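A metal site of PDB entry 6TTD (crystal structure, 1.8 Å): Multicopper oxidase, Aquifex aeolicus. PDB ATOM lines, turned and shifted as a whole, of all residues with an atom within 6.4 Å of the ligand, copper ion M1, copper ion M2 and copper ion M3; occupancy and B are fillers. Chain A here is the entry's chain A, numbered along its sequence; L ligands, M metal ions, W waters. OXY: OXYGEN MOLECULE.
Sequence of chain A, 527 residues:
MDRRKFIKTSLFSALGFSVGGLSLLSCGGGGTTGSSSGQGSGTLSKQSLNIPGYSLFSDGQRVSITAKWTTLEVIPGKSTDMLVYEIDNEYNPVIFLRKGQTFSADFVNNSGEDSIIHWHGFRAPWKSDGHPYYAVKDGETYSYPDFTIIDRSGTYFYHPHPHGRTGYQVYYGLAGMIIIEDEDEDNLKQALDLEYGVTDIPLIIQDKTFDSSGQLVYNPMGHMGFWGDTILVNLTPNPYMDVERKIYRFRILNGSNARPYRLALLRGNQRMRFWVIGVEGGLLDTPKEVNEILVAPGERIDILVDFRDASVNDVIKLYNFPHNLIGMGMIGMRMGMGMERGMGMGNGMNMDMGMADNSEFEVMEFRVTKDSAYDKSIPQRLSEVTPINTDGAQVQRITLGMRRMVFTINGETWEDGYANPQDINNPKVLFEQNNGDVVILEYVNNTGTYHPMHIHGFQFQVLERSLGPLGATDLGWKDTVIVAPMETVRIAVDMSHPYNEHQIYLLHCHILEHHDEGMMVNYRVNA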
ATOM      1  N   HIS A 118       1.704 -16.530 -13.542  1.00  0.00           N
ATOM      2  CA  HIS A 118       1.665 -15.074 -13.504  1.00  0.00           C
ATOM      3  C   HIS A 118       0.239 -14.611 -13.170  1.00  0.00           C
ATOM      4  O   HIS A 118      -0.752 -15.196 -13.655  1.00  0.00           O
ATOM      5  CB  HIS A 118       2.113 -14.528 -14.879  1.00  0.00           C
ATOM      6  CG  HIS A 118       1.760 -13.085 -15.147  1.00  0.00           C
ATOM      7  ND1 HIS A 118       2.255 -12.047 -14.402  1.00  0.00           N
ATOM      8  CD2 HIS A 118       0.982 -12.527 -16.099  1.00  0.00           C
ATOM      9  CE1 HIS A 118       1.793 -10.907 -14.877  1.00  0.00           C
ATOM     10  NE2 HIS A 118       1.010 -11.171 -15.904  1.00  0.00           N
ATOM     11  N   TRP A 119       0.126 -13.598 -12.302  1.00  0.00           N
ATOM     12  CA  TRP A 119      -1.168 -13.050 -11.897  1.00  0.00           C
ATOM     13  C   TRP A 119      -1.372 -11.842 -12.802  1.00  0.00           C
ATOM     14  O   TRP A 119      -0.932 -10.736 -12.520  1.00  0.00           O
ATOM     15  CB  TRP A 119      -1.192 -12.678 -10.413  1.00  0.00           C
ATOM     16  CG  TRP A 119      -0.336 -13.615  -9.622  1.00  0.00           C
ATOM     17  CD1 TRP A 119       0.924 -13.354  -9.115  1.00  0.00           C
ATOM     18  CD2 TRP A 119      -0.625 -14.995  -9.265  1.00  0.00           C
ATOM     19  NE1 TRP A 119       1.418 -14.507  -8.462  1.00  0.00           N
ATOM     20  CE2 TRP A 119       0.485 -15.503  -8.548  1.00  0.00           C
ATOM     21  CE3 TRP A 119      -1.733 -15.842  -9.474  1.00  0.00           C
ATOM     22  CZ2 TRP A 119       0.512 -16.798  -8.047  1.00  0.00           C
ATOM     23  CZ3 TRP A 119      -1.691 -17.155  -8.944  1.00  0.00           C
ATOM     24  CH2 TRP A 119      -0.588 -17.600  -8.260  1.00  0.00           C
ATOM     25  N   HIS A 120      -2.008 -12.069 -13.931  1.00  0.00           N
ATOM     26  CA  HIS A 120      -2.073 -11.018 -14.948  1.00  0.00           C
ATOM     27  C   HIS A 120      -2.995  -9.883 -14.455  1.00  0.00           C
ATOM     28  O   HIS A 120      -4.175 -10.097 -14.174  1.00  0.00           O
ATOM     29  CB  HIS A 120      -2.512 -11.633 -16.296  1.00  0.00           C
ATOM     30  CG  HIS A 120      -2.761 -10.626 -17.383  1.00  0.00           C
ATOM     31  ND1 HIS A 120      -2.539 -10.932 -18.719  1.00  0.00           N
ATOM     32  CD2 HIS A 120      -3.254  -9.362 -17.373  1.00  0.00           C
ATOM     33  CE1 HIS A 120      -2.874  -9.893 -19.475  1.00  0.00           C
ATOM     34  NE2 HIS A 120      -3.295  -8.930 -18.689  1.00  0.00           N
ATOM     35  N   GLY A 121      -2.429  -8.659 -14.337  1.00  0.00           N
ATOM     36  CA  GLY A 121      -3.133  -7.485 -13.843  1.00  0.00           C
ATOM     37  C   GLY A 121      -2.701  -7.065 -12.452  1.00  0.00           C
ATOM     38  O   GLY A 121      -2.966  -5.933 -12.076  1.00  0.00           O
ATOM     39  N   ASP A 129       5.550 -11.920  -9.224  1.00  0.00           N
ATOM     40  CA  ASP A 129       4.762 -11.643 -10.422  1.00  0.00           C
ATOM     41  C   ASP A 129       4.708 -12.832 -11.376  1.00  0.00           C
ATOM     42  O   ASP A 129       3.798 -12.914 -12.201  1.00  0.00           O
ATOM     43  CB  ASP A 129       5.375 -10.396 -11.091  1.00  0.00           C
ATOM     44  CG  ASP A 129       4.748 -10.022 -12.388  1.00  0.00           C
ATOM     45  OD1 ASP A 129       3.504  -9.922 -12.463  1.00  0.00           O
ATOM     46  OD2 ASP A 129       5.495  -9.746 -13.374  1.00  0.00           O
ATOM     47  N   PHE A 157      -6.623 -12.468 -14.072  1.00  0.00           N
ATOM     48  CA  PHE A 157      -6.356 -13.619 -14.951  1.00  0.00           C
ATOM     49  C   PHE A 157      -5.092 -14.327 -14.478  1.00  0.00           C
ATOM     50  O   PHE A 157      -4.031 -13.673 -14.401  1.00  0.00           O
ATOM     51  CB  PHE A 157      -6.206 -13.046 -16.388  1.00  0.00           C
ATOM     52  CG  PHE A 157      -5.936 -14.049 -17.528  1.00  0.00           C
ATOM     53  CD1 PHE A 157      -6.172 -15.419 -17.423  1.00  0.00           C
ATOM     54  CD2 PHE A 157      -5.494 -13.522 -18.770  1.00  0.00           C
ATOM     55  CE1 PHE A 157      -5.922 -16.279 -18.518  1.00  0.00           C
ATOM     56  CE2 PHE A 157      -5.242 -14.355 -19.852  1.00  0.00           C
ATOM     57  CZ  PHE A 157      -5.463 -15.746 -19.727  1.00  0.00           C
ATOM     58  N   HIS A 159      -2.309 -17.392 -15.254  1.00  0.00           N
ATOM     59  CA  HIS A 159      -1.921 -18.300 -16.317  1.00  0.00           C
ATOM     60  C   HIS A 159      -0.398 -18.464 -16.296  1.00  0.00           C
ATOM     61  O   HIS A 159       0.289 -17.659 -15.673  1.00  0.00           O
ATOM     62  CB  HIS A 159      -2.411 -17.780 -17.680  1.00  0.00           C
ATOM     63  CG  HIS A 159      -1.739 -16.533 -18.152  1.00  0.00           C
ATOM     64  ND1 HIS A 159      -0.428 -16.515 -18.586  1.00  0.00           N
ATOM     65  CD2 HIS A 159      -2.200 -15.264 -18.331  1.00  0.00           C
ATOM     66  CE1 HIS A 159      -0.094 -15.290 -18.981  1.00  0.00           C
ATOM     67  NE2 HIS A 159      -1.158 -14.514 -18.850  1.00  0.00           N
ATOM     68  N   PRO A 160       0.145 -19.502 -16.959  1.00  0.00           N
ATOM     69  CA  PRO A 160       1.602 -19.729 -16.913  1.00  0.00           C
ATOM     70  C   PRO A 160       2.385 -18.707 -17.753  1.00  0.00           C
ATOM     71  O   PRO A 160       1.835 -18.041 -18.641  1.00  0.00           O
ATOM     72  CB  PRO A 160       1.771 -21.135 -17.515  1.00  0.00           C
ATOM     73  CG  PRO A 160       0.565 -21.270 -18.440  1.00  0.00           C
ATOM     74  CD  PRO A 160      -0.570 -20.533 -17.731  1.00  0.00           C
ATOM     75  N   HIS A 161       3.690 -18.632 -17.486  1.00  0.00           N
ATOM     76  CA  HIS A 161       4.501 -17.642 -18.195  1.00  0.00           C
ATOM     77  C   HIS A 161       5.913 -18.169 -18.509  1.00  0.00           C
ATOM     78  O   HIS A 161       6.870 -17.367 -18.461  1.00  0.00           O
ATOM     79  CB  HIS A 161       4.582 -16.361 -17.311  1.00  0.00           C
ATOM     80  CG  HIS A 161       4.512 -15.083 -18.097  1.00  0.00           C
ATOM     81  ND1 HIS A 161       5.504 -14.687 -18.970  1.00  0.00           N
ATOM     82  CD2 HIS A 161       3.569 -14.102 -18.128  1.00  0.00           C
ATOM     83  CE1 HIS A 161       5.155 -13.533 -19.522  1.00  0.00           C
ATOM     84  NE2 HIS A 161       3.996 -13.139 -19.008  1.00  0.00           N
ATOM     85  N   THR A 166       4.571 -20.404 -23.295  1.00  0.00           N
ATOM     86  CA  THR A 166       3.335 -19.928 -22.679  1.00  0.00           C
ATOM     87  C   THR A 166       2.133 -20.261 -23.548  1.00  0.00           C
ATOM     88  O   THR A 166       1.069 -20.605 -23.019  1.00  0.00           O
ATOM     89  CB  THR A 166       3.433 -18.416 -22.412  1.00  0.00           C
ATOM     90  OG1 THR A 166       4.382 -18.224 -21.375  1.00  0.00           O
ATOM     91  CG2 THR A 166       2.081 -17.817 -21.945  1.00  0.00           C
ATOM     92  N   GLY A 298      -5.865 -11.349 -23.315  1.00  0.00           N
ATOM     93  CA  GLY A 298      -5.374 -10.575 -22.205  1.00  0.00           C
ATOM     94  C   GLY A 298      -6.343  -9.529 -21.709  1.00  0.00           C
ATOM     95  O   GLY A 298      -6.252  -9.144 -20.545  1.00  0.00           O
ATOM     96  N   HIS A 454       0.783  -5.521 -23.657  1.00  0.00           N
ATOM     97  CA  HIS A 454       0.522  -5.668 -22.237  1.00  0.00           C
ATOM     98  C   HIS A 454       1.794  -5.281 -21.484  1.00  0.00           C
ATOM     99  O   HIS A 454       2.908  -5.591 -21.946  1.00  0.00           O
ATOM    100  CB  HIS A 454       0.100  -7.124 -21.986  1.00  0.00           C
ATOM    101  CG  HIS A 454       0.060  -7.500 -20.549  1.00  0.00           C
ATOM    102  ND1 HIS A 454      -0.710  -6.814 -19.623  1.00  0.00           N
ATOM    103  CD2 HIS A 454       0.672  -8.521 -19.863  1.00  0.00           C
ATOM    104  CE1 HIS A 454      -0.565  -7.386 -18.439  1.00  0.00           C
ATOM    105  NE2 HIS A 454       0.287  -8.406 -18.565  1.00  0.00           N
ATOM    106  N   ILE A 455       1.656  -4.596 -20.350  1.00  0.00           N
ATOM    107  CA  ILE A 455       2.773  -4.407 -19.421  1.00  0.00           C
ATOM    108  C   ILE A 455       2.418  -5.059 -18.107  1.00  0.00           C
ATOM    109  O   ILE A 455       1.265  -5.010 -17.667  1.00  0.00           O
ATOM    110  CB  ILE A 455       3.183  -2.932 -19.192  1.00  0.00           C
ATOM    111  CG1 ILE A 455       2.008  -2.120 -18.576  1.00  0.00           C
ATOM    112  CG2 ILE A 455       3.655  -2.290 -20.501  1.00  0.00           C
ATOM    113  CD1 ILE A 455       2.367  -0.621 -18.212  1.00  0.00           C
ATOM    114  N   HIS A 456       3.413  -5.703 -17.495  1.00  0.00           N
ATOM    115  CA  HIS A 456       3.285  -6.132 -16.103  1.00  0.00           C
ATOM    116  C   HIS A 456       3.475  -4.908 -15.188  1.00  0.00           C
ATOM    117  O   HIS A 456       4.026  -3.861 -15.606  1.00  0.00           O
ATOM    118  CB  HIS A 456       4.350  -7.192 -15.778  1.00  0.00           C
ATOM    119  CG  HIS A 456       4.188  -8.487 -16.518  1.00  0.00           C
ATOM    120  ND1 HIS A 456       4.598  -9.705 -15.979  1.00  0.00           N
ATOM    121  CD2 HIS A 456       3.690  -8.755 -17.745  1.00  0.00           C
ATOM    122  CE1 HIS A 456       4.355 -10.671 -16.869  1.00  0.00           C
ATOM    123  NE2 HIS A 456       3.808 -10.116 -17.943  1.00  0.00           N
ATOM    124  N   GLY A 457       3.062  -5.058 -13.932  1.00  0.00           N
ATOM    125  CA  GLY A 457       3.422  -4.147 -12.861  1.00  0.00           C
ATOM    126  C   GLY A 457       2.457  -3.032 -12.599  1.00  0.00           C
ATOM    127  O   GLY A 457       2.262  -2.662 -11.441  1.00  0.00           O
ATOM    128  N   ASP A 479      -4.762  -2.794 -18.852  1.00  0.00           N
ATOM    129  CA  ASP A 479      -3.435  -3.406 -18.797  1.00  0.00           C
ATOM    130  C   ASP A 479      -3.017  -4.078 -20.106  1.00  0.00           C
ATOM    131  O   ASP A 479      -1.840  -4.447 -20.234  1.00  0.00           O
ATOM    132  CB  ASP A 479      -3.286  -4.365 -17.590  1.00  0.00           C
ATOM    133  CG  ASP A 479      -3.967  -5.728 -17.790  1.00  0.00           C
ATOM    134  OD1 ASP A 479      -4.005  -6.266 -18.929  1.00  0.00           O
ATOM    135  OD2 ASP A 479      -4.464  -6.265 -16.774  1.00  0.00           O
ATOM    136  N   THR A 480      -3.923  -4.165 -21.099  1.00  0.00           N
ATOM    137  CA  THR A 480      -3.639  -4.658 -22.451  1.00  0.00           C
ATOM    138  C   THR A 480      -4.354  -3.768 -23.475  1.00  0.00           C
ATOM    139  O   THR A 480      -5.563  -3.543 -23.355  1.00  0.00           O
ATOM    140  CB  THR A 480      -4.134  -6.092 -22.597  1.00  0.00           C
ATOM    141  OG1 THR A 480      -3.452  -6.901 -21.625  1.00  0.00           O
ATOM    142  CG2 THR A 480      -3.842  -6.607 -23.983  1.00  0.00           C
ATOM    143  N   LEU A 506       7.825  -7.052 -17.256  1.00  0.00           N
ATOM    144  CA  LEU A 506       7.792  -7.334 -18.692  1.00  0.00           C
ATOM    145  C   LEU A 506       6.924  -6.322 -19.445  1.00  0.00           C
ATOM    146  O   LEU A 506       5.952  -5.782 -18.917  1.00  0.00           O
ATOM    147  CB  LEU A 506       7.215  -8.732 -18.944  1.00  0.00           C
ATOM    148  CG  LEU A 506       8.052  -9.814 -18.298  1.00  0.00           C
ATOM    149  CD1 LEU A 506       7.348 -11.093 -18.519  1.00  0.00           C
ATOM    150  CD2 LEU A 506       9.379  -9.833 -19.057  1.00  0.00           C
ATOM    151  N   HIS A 508       5.151  -6.795 -23.300  1.00  0.00           N
ATOM    152  CA  HIS A 508       5.163  -7.771 -24.382  1.00  0.00           C
ATOM    153  C   HIS A 508       3.803  -7.850 -25.067  1.00  0.00           C
ATOM    154  O   HIS A 508       2.793  -7.319 -24.593  1.00  0.00           O
ATOM    155  CB  HIS A 508       5.543  -9.173 -23.869  1.00  0.00           C
ATOM    156  CG  HIS A 508       4.530  -9.794 -22.935  1.00  0.00           C
ATOM    157  ND1 HIS A 508       3.422 -10.517 -23.376  1.00  0.00           N
ATOM    158  CD2 HIS A 508       4.509  -9.865 -21.577  1.00  0.00           C
ATOM    159  CE1 HIS A 508       2.754 -10.967 -22.323  1.00  0.00           C
ATOM    160  NE2 HIS A 508       3.393 -10.605 -21.219  1.00  0.00           N
ATOM    161  N   CYS A 509       3.810  -8.509 -26.213  1.00  0.00           N
ATOM    162  CA  CYS A 509       2.579  -8.786 -26.935  1.00  0.00           C
ATOM    163  C   CYS A 509       1.849  -9.947 -26.276  1.00  0.00           C
ATOM    164  O   CYS A 509       2.472 -10.923 -25.806  1.00  0.00           O
ATOM    165  CB  CYS A 509       2.899  -9.103 -28.405  1.00  0.00           C
ATOM    166  SG  CYS A 509       1.446  -9.429 -29.336  1.00  0.00           S
ATOM    167  N   HIS A 510       0.510  -9.849 -26.223  1.00  0.00           N
ATOM    168  CA  HIS A 510      -0.252 -10.932 -25.625  1.00  0.00           C
ATOM    169  C   HIS A 510      -0.860 -11.885 -26.656  1.00  0.00           C
ATOM    170  O   HIS A 510      -1.691 -12.712 -26.300  1.00  0.00           O
ATOM    171  CB  HIS A 510      -1.327 -10.378 -24.710  1.00  0.00           C
ATOM    172  CG  HIS A 510      -1.647 -11.293 -23.569  1.00  0.00           C
ATOM    173  ND1 HIS A 510      -2.365 -12.453 -23.726  1.00  0.00           N
ATOM    174  CD2 HIS A 510      -1.335 -11.217 -22.245  1.00  0.00           C
ATOM    175  CE1 HIS A 510      -2.507 -13.040 -22.547  1.00  0.00           C
ATOM    176  NE2 HIS A 510      -1.898 -12.305 -21.634  1.00  0.00           N
ATOM    177  N   LEU A 512       0.012 -15.086 -27.734  1.00  0.00           N
ATOM    178  CA  LEU A 512       0.944 -15.956 -27.000  1.00  0.00           C
ATOM    179  C   LEU A 512       2.045 -16.565 -27.905  1.00  0.00           C
ATOM    180  O   LEU A 512       3.189 -16.738 -27.445  1.00  0.00           O
ATOM    181  CB  LEU A 512       0.171 -17.046 -26.264  1.00  0.00           C
ATOM    182  CG  LEU A 512      -0.840 -16.541 -25.229  1.00  0.00           C
ATOM    183  CD1 LEU A 512      -1.442 -17.759 -24.431  1.00  0.00           C
ATOM    184  CD2 LEU A 512      -0.286 -15.503 -24.287  1.00  0.00           C
ATOM    185  N   HIS A 515       4.547 -13.722 -28.084  1.00  0.00           N
ATOM    186  CA  HIS A 515       5.292 -13.814 -26.826  1.00  0.00           C
ATOM    187  C   HIS A 515       6.320 -14.941 -26.897  1.00  0.00           C
ATOM    188  O   HIS A 515       7.511 -14.717 -26.650  1.00  0.00           O
ATOM    189  CB  HIS A 515       4.337 -14.027 -25.630  1.00  0.00           C
ATOM    190  CG  HIS A 515       5.028 -14.479 -24.384  1.00  0.00           C
ATOM    191  ND1 HIS A 515       5.408 -15.794 -24.176  1.00  0.00           N
ATOM    192  CD2 HIS A 515       5.443 -13.799 -23.293  1.00  0.00           C
ATOM    193  CE1 HIS A 515       6.024 -15.901 -23.012  1.00  0.00           C
ATOM    194  NE2 HIS A 515       6.059 -14.698 -22.458  1.00  0.00           N
ATOM    195  N   MET A 520       8.937  -9.520 -26.613  1.00  0.00           N
ATOM    196  CA  MET A 520       8.884  -9.302 -25.165  1.00  0.00           C
ATOM    197  C   MET A 520      10.209  -8.682 -24.750  1.00  0.00           C
ATOM    198  O   MET A 520      11.246  -9.046 -25.298  1.00  0.00           O
ATOM    199  CB  MET A 520       8.689 -10.632 -24.444  1.00  0.00           C
ATOM    200  CG  MET A 520       8.835 -10.567 -22.964  1.00  0.00           C
ATOM    201  SD  MET A 520       8.366 -12.148 -22.115  1.00  0.00           S
ATOM    202  CE  MET A 520       9.423 -13.336 -22.947  1.00  0.00           C
HETATM  203  O1  OXY L   1       0.995 -12.192 -19.794  1.00  0.00           O
HETATM  204  O2  OXY L   1       0.510 -11.589 -19.011  1.00  0.00           O
HETATM  205 CU    CU M   1       3.109 -11.388 -19.322  1.00  0.00          CU
HETATM  206 CU    CU M   2       0.647  -9.850 -17.341  1.00  0.00          CU
HETATM  207 CU    CU M   3      -1.682 -12.632 -19.475  1.00  0.00          CU
HETATM  208  O   HOH W   1       0.241  -7.771 -15.082  1.00  0.00           O
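NE2 of His 120 sits at hydrogen-bond distance from OD1 of Asp 479 (2.8 Å).
N of His 456 is in hydrogen-bond range of O of Leu 506 (2.9 Å).
ND1 of His 454 lies close to NE2 of His 120, at 3.5 Å.
A ring nitrogen (ND1) of His 454 is in hydrogen-bond range of the side-chain hydroxyl (OG1) of Thr 480 (3.4 Å).
ND1 of His 456 sits at hydrogen-bond distance from OD2 of Asp 129 (2.8 Å).
A ring nitrogen (ND1) of His 118 lies within hydrogen-bond range of the backbone carbonyl oxygen (O) of Asp 129.
The backbone carbonyl oxygen (O) of His 159 is in hydrogen-bond range of the backbone NH (N) of His 118 (2.8 Å).
The backbone carbonyl oxygen (O) of Gly 298 lies within hydrogen-bond range of a ring nitrogen (NE2) of His 120.
Hydrophobic or aromatic side chains within 4 Å of the ligand: His 118, His 120, His 159, His 161, His 454, His 508 and His 510.
Along chain A the residues within 4 Å of the ligand span positions 118 to 510.
Within 4 Å of copper ion M1: His 161, His 454, His 456 and His 508.
Along chain A the residues within 4 Å of copper ion M1 span positions 161 to 508.
Copper ion M3 is bound by ND1 of His 120, 2.0 Å away.
Copper ion M3 is bound by NE2 of His 159 (2.1 Å).
NE2 of His 510 is bound to copper ion M3 (2.2 Å).
O2 of the ligand is bound to copper ion M3.
Copper ion M1 is bound by NE2 of His 161 (2.0 Å).
A ring nitrogen (NE2) of His 456 binds copper ion M1, at 2.0 Å.
A ring nitrogen (NE2) of His 508 binds copper ion M1 (2.1 Å).
Copper ion M1 is bound by an oxygen (O1) of the ligand (2.3 Å).
Copper ion M1 has four donor atoms within binding distance.
Phe 157 touches copper ion M3.
Within 4 Å of copper ion M3: His 120, Phe 157, His 159 and His 510.
Along chain A the residues within 4 Å of copper ion M3 span positions 120 to 510.
The nearest printed residue that does not touch copper ion M3 is His 118 (4.3 Å).
Copper ion M2 is bound by a ring nitrogen (NE2) of His 454 (1.9 Å).
NE2 of His 118 is bound to copper ion M2 (2.0 Å).
Copper ion M2 is bound by O2 of the ligand (2.4 Å).
Of the 24 residues printed, 4 come within 4 Å of copper ion M2.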
